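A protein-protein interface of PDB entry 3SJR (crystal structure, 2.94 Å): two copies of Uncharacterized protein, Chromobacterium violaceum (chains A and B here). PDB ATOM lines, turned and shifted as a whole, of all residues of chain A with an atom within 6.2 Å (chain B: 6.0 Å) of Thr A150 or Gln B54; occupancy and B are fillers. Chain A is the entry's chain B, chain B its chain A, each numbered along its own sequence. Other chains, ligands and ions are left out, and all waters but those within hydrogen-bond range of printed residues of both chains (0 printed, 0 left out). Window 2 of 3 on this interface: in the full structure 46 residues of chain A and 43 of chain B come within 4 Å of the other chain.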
ATOM      1  N   LEU A 143       3.389   8.799   8.904  1.00  0.00           N
ATOM      2  CA  LEU A 143       3.818   7.447   8.649  1.00  0.00           C
ATOM      3  C   LEU A 143       4.601   6.880   9.824  1.00  0.00           C
ATOM      4  O   LEU A 143       4.497   5.695  10.121  1.00  0.00           O
ATOM      5  CB  LEU A 143       4.603   7.376   7.345  1.00  0.00           C
ATOM      6  CG  LEU A 143       3.690   7.442   6.112  1.00  0.00           C
ATOM      7  CD1 LEU A 143       4.465   7.795   4.883  1.00  0.00           C
ATOM      8  CD2 LEU A 143       2.909   6.153   5.880  1.00  0.00           C
ATOM      9  N   VAL A 148       4.048   2.751  10.815  1.00  0.00           N
ATOM     10  CA  VAL A 148       3.786   2.104   9.542  1.00  0.00           C
ATOM     11  C   VAL A 148       4.829   2.533   8.483  1.00  0.00           C
ATOM     12  O   VAL A 148       4.625   2.357   7.278  1.00  0.00           O
ATOM     13  CB  VAL A 148       2.291   2.334   9.121  1.00  0.00           C
ATOM     14  CG1 VAL A 148       2.070   3.759   8.621  1.00  0.00           C
ATOM     15  CG2 VAL A 148       1.807   1.289   8.102  1.00  0.00           C
ATOM     16  N   TYR A 149       5.964   3.047   8.965  1.00  0.00           N
ATOM     17  CA  TYR A 149       7.054   3.577   8.128  1.00  0.00           C
ATOM     18  C   TYR A 149       8.155   2.536   7.813  1.00  0.00           C
ATOM     19  O   TYR A 149       9.276   2.631   8.328  1.00  0.00           O
ATOM     20  CB  TYR A 149       7.649   4.816   8.823  1.00  0.00           C
ATOM     21  CG  TYR A 149       8.523   5.727   7.975  1.00  0.00           C
ATOM     22  CD1 TYR A 149       8.017   6.372   6.840  1.00  0.00           C
ATOM     23  CD2 TYR A 149       9.843   5.985   8.335  1.00  0.00           C
ATOM     24  CE1 TYR A 149       8.821   7.229   6.069  1.00  0.00           C
ATOM     25  CE2 TYR A 149      10.652   6.844   7.576  1.00  0.00           C
ATOM     26  CZ  TYR A 149      10.136   7.464   6.447  1.00  0.00           C
ATOM     27  OH  TYR A 149      10.935   8.306   5.696  1.00  0.00           O
ATOM     28  N   THR A 150       7.822   1.558   6.964  1.00  0.00           N
ATOM     29  CA  THR A 150       8.740   0.487   6.536  1.00  0.00           C
ATOM     30  C   THR A 150       9.950   1.052   5.805  1.00  0.00           C
ATOM     31  O   THR A 150       9.839   2.077   5.132  1.00  0.00           O
ATOM     32  CB  THR A 150       8.065  -0.483   5.523  1.00  0.00           C
ATOM     33  OG1 THR A 150       6.722  -0.759   5.918  1.00  0.00           O
ATOM     34  CG2 THR A 150       8.825  -1.808   5.405  1.00  0.00           C
ATOM     35  N   PRO A 151      11.111   0.374   5.912  1.00  0.00           N
ATOM     36  CA  PRO A 151      12.199   0.696   4.995  1.00  0.00           C
ATOM     37  C   PRO A 151      11.682   0.767   3.563  1.00  0.00           C
ATOM     38  O   PRO A 151      12.010   1.706   2.841  1.00  0.00           O
ATOM     39  CB  PRO A 151      13.168  -0.487   5.163  1.00  0.00           C
ATOM     40  CG  PRO A 151      12.457  -1.475   6.053  1.00  0.00           C
ATOM     41  CD  PRO A 151      11.512  -0.671   6.865  1.00  0.00           C
ATOM     42  N   ALA A 152      10.858  -0.211   3.184  1.00  0.00           N
ATOM     43  CA  ALA A 152      10.221  -0.247   1.870  1.00  0.00           C
ATOM     44  C   ALA A 152       9.405   1.023   1.599  1.00  0.00           C
ATOM     45  O   ALA A 152       9.610   1.686   0.579  1.00  0.00           O
ATOM     46  CB  ALA A 152       9.361  -1.501   1.730  1.00  0.00           C
ATOM     47  N   VAL A 153       8.517   1.374   2.530  1.00  0.00           N
ATOM     48  CA  VAL A 153       7.653   2.544   2.383  1.00  0.00           C
ATOM     49  C   VAL A 153       8.455   3.815   2.191  1.00  0.00           C
ATOM     50  O   VAL A 153       8.215   4.559   1.239  1.00  0.00           O
ATOM     51  CB  VAL A 153       6.728   2.747   3.594  1.00  0.00           C
ATOM     52  CG1 VAL A 153       6.143   4.155   3.572  1.00  0.00           C
ATOM     53  CG2 VAL A 153       5.603   1.724   3.607  1.00  0.00           C
ATOM     54  N   ALA A 154       9.393   4.048   3.112  1.00  0.00           N
ATOM     55  CA  ALA A 154      10.271   5.222   3.123  1.00  0.00           C
ATOM     56  C   ALA A 154      10.942   5.423   1.775  1.00  0.00           C
ATOM     57  O   ALA A 154      10.844   6.495   1.171  1.00  0.00           O
ATOM     58  CB  ALA A 154      11.312   5.080   4.199  1.00  0.00           C
ATOM     59  N   GLY A 155      11.604   4.372   1.309  1.00  0.00           N
ATOM     60  CA  GLY A 155      12.223   4.360  -0.002  1.00  0.00           C
ATOM     61  C   GLY A 155      11.232   4.659  -1.104  1.00  0.00           C
ATOM     62  O   GLY A 155      11.548   5.401  -2.021  1.00  0.00           O
ATOM     63  N   GLN A 156      10.031   4.093  -1.024  1.00  0.00           N
ATOM     64  CA  GLN A 156       9.023   4.361  -2.046  1.00  0.00           C
ATOM     65  C   GLN A 156       8.696   5.861  -2.048  1.00  0.00           C
ATOM     66  O   GLN A 156       8.633   6.506  -3.097  1.00  0.00           O
ATOM     67  CB  GLN A 156       7.770   3.504  -1.832  1.00  0.00           C
ATOM     68  CG  GLN A 156       6.683   3.776  -2.854  1.00  0.00           C
ATOM     69  CD  GLN A 156       5.982   2.509  -3.377  1.00  0.00           C
ATOM     70  OE1 GLN A 156       5.246   1.819  -2.645  1.00  0.00           O
ATOM     71  NE2 GLN A 156       6.192   2.214  -4.664  1.00  0.00           N
ATOM     72  N   SER B  51       0.178  -5.074  -1.922  1.00  0.00           N
ATOM     73  CA  SER B  51       0.249  -3.812  -1.161  1.00  0.00           C
ATOM     74  C   SER B  51       0.776  -2.630  -1.986  1.00  0.00           C
ATOM     75  O   SER B  51       1.753  -1.958  -1.617  1.00  0.00           O
ATOM     76  CB  SER B  51       1.051  -3.977   0.137  1.00  0.00           C
ATOM     77  OG  SER B  51       2.401  -3.574  -0.038  1.00  0.00           O
ATOM     78  N   LEU B  52       0.116  -2.394  -3.117  1.00  0.00           N
ATOM     79  CA  LEU B  52       0.198  -1.120  -3.819  1.00  0.00           C
ATOM     80  C   LEU B  52      -0.585  -0.164  -2.951  1.00  0.00           C
ATOM     81  O   LEU B  52      -0.479   1.056  -3.071  1.00  0.00           O
ATOM     82  CB  LEU B  52      -0.470  -1.231  -5.189  1.00  0.00           C
ATOM     83  CG  LEU B  52       0.176  -2.154  -6.226  1.00  0.00           C
ATOM     84  CD1 LEU B  52      -0.863  -2.670  -7.216  1.00  0.00           C
ATOM     85  CD2 LEU B  52       1.337  -1.460  -6.946  1.00  0.00           C
ATOM     86  N   SER B  53      -1.386  -0.776  -2.083  1.00  0.00           N
ATOM     87  CA  SER B  53      -2.153  -0.137  -1.029  1.00  0.00           C
ATOM     88  C   SER B  53      -1.313   0.737  -0.087  1.00  0.00           C
ATOM     89  O   SER B  53      -1.745   1.818   0.309  1.00  0.00           O
ATOM     90  CB  SER B  53      -2.882  -1.224  -0.234  1.00  0.00           C
ATOM     91  OG  SER B  53      -3.566  -0.686   0.880  1.00  0.00           O
ATOM     92  N   GLN B  54      -0.121   0.281   0.281  1.00  0.00           N
ATOM     93  CA  GLN B  54       0.731   1.111   1.126  1.00  0.00           C
ATOM     94  C   GLN B  54       1.491   2.160   0.309  1.00  0.00           C
ATOM     95  O   GLN B  54       1.996   3.136   0.859  1.00  0.00           O
ATOM     96  CB  GLN B  54       1.648   0.273   2.025  1.00  0.00           C
ATOM     97  CG  GLN B  54       2.809  -0.394   1.322  1.00  0.00           C
ATOM     98  CD  GLN B  54       3.540  -1.371   2.227  1.00  0.00           C
ATOM     99  OE1 GLN B  54       2.945  -2.320   2.743  1.00  0.00           O
ATOM    100  NE2 GLN B  54       4.839  -1.148   2.415  1.00  0.00           N
ATOM    101  N   GLY B  55       1.551   1.958  -1.003  1.00  0.00           N
ATOM    102  CA  GLY B  55       2.036   2.982  -1.920  1.00  0.00           C
ATOM    103  C   GLY B  55       1.023   4.103  -2.038  1.00  0.00           C
ATOM    104  O   GLY B  55       1.359   5.272  -1.921  1.00  0.00           O
ATOM    105  N   ALA B  56      -0.235   3.741  -2.251  1.00  0.00           N
ATOM    106  CA  ALA B  56      -1.309   4.726  -2.393  1.00  0.00           C
ATOM    107  C   ALA B  56      -1.390   5.688  -1.210  1.00  0.00           C
ATOM    108  O   ALA B  56      -1.485   6.892  -1.391  1.00  0.00           O
ATOM    109  CB  ALA B  56      -2.647   4.036  -2.621  1.00  0.00           C
ATOM    110  N   GLN B  57      -1.331   5.139  -0.006  1.00  0.00           N
ATOM    111  CA  GLN B  57      -1.394   5.915   1.232  1.00  0.00           C
ATOM    112  C   GLN B  57      -0.248   6.924   1.358  1.00  0.00           C
ATOM    113  O   GLN B  57      -0.437   8.049   1.825  1.00  0.00           O
ATOM    114  CB  GLN B  57      -1.380   4.950   2.419  1.00  0.00           C
ATOM    115  CG  GLN B  57      -1.058   5.580   3.764  1.00  0.00           C
ATOM    116  CD  GLN B  57      -0.497   4.566   4.735  1.00  0.00           C
ATOM    117  OE1 GLN B  57       0.575   3.980   4.506  1.00  0.00           O
ATOM    118  NE2 GLN B  57      -1.216   4.345   5.826  1.00  0.00           N
ATOM    119  N   ALA B  58       0.937   6.498   0.942  1.00  0.00           N
ATOM    120  CA  ALA B  58       2.102   7.350   0.957  1.00  0.00           C
ATOM    121  C   ALA B  58       1.820   8.543   0.072  1.00  0.00           C
ATOM    122  O   ALA B  58       1.837   9.687   0.528  1.00  0.00           O
ATOM    123  CB  ALA B  58       3.333   6.583   0.452  1.00  0.00           C
ATOM    124  N   ALA B  59       1.523   8.252  -1.190  1.00  0.00           N
ATOM    125  CA  ALA B  59       1.303   9.267  -2.198  1.00  0.00           C
ATOM    126  C   ALA B  59       0.227  10.251  -1.778  1.00  0.00           C
ATOM    127  O   ALA B  59       0.317  11.425  -2.092  1.00  0.00           O
ATOM    128  CB  ALA B  59       0.935   8.615  -3.512  1.00  0.00           C
ATOM    129  N   VAL B 142      -8.747   1.567   0.046  1.00  0.00           N
ATOM    130  CA  VAL B 142      -7.376   1.600   0.566  1.00  0.00           C
ATOM    131  C   VAL B 142      -7.268   1.214   2.037  1.00  0.00           C
ATOM    132  O   VAL B 142      -6.387   0.447   2.412  1.00  0.00           O
ATOM    133  CB  VAL B 142      -6.754   3.001   0.401  1.00  0.00           C
ATOM    134  CG1 VAL B 142      -5.330   3.012   0.926  1.00  0.00           C
ATOM    135  CG2 VAL B 142      -6.789   3.438  -1.061  1.00  0.00           C
ATOM    136  N   LEU B 146      -5.669  -1.752   3.768  1.00  0.00           N
ATOM    137  CA  LEU B 146      -4.560  -1.551   4.698  1.00  0.00           C
ATOM    138  C   LEU B 146      -4.880  -2.201   6.029  1.00  0.00           C
ATOM    139  O   LEU B 146      -4.062  -2.181   6.945  1.00  0.00           O
ATOM    140  CB  LEU B 146      -4.254  -0.058   4.905  1.00  0.00           C
ATOM    141  CG  LEU B 146      -3.342   0.675   3.911  1.00  0.00           C
ATOM    142  CD1 LEU B 146      -3.227   2.129   4.298  1.00  0.00           C
ATOM    143  CD2 LEU B 146      -1.949   0.051   3.804  1.00  0.00           C
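OG of Ser B51 lies within hydrogen-bond range of OE1 of Gln B54 (3.1 Å). The backbone carbonyl oxygen (O) of Leu A143 sits at hydrogen-bond distance from the backbone NH (N) of Val A148, 3.1 Å away. O of Leu A143 lies within hydrogen-bond range of N of Tyr A149 (3.2 Å).
Of the 11 printed residues of chain B, 3 touch a printed residue of chain A. Among the printed residues, 4 pairs touch across the chains. Among the printed residues, no Asp or Glu carboxylate lies within 4 Å of a Lys or Arg side-chain nitrogen of the other chain.
Of the printed residues of chain B, Thr A150 touches Gln B54. Of the printed residues of chain A, Gln B54 touches Thr A150 and Val A153. Of the printed residues of chain B, Val A153 touches Gln B54. Printed residues of chain A within 4 Å of Gln B57: Leu A143 (3.5 Å). Printed residues of chain B within 4 Å of Leu A143: Gln B57 (3.5 Å). Printed residues of chain A within 4 Å of Gly B55: Gln A156. Leu B52 touches none of the printed residues of chain A.
No position is printed for both chains.
Among the printed residues, pairs that only touch across the chains: Leu A143 with Gln B57 (3.5 Å), Thr A150 with Gln B54 (3.996 Å), Val A153 with Gln B54 (3.2 Å) and Gln A156 with Gly B55 (3.5 Å).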
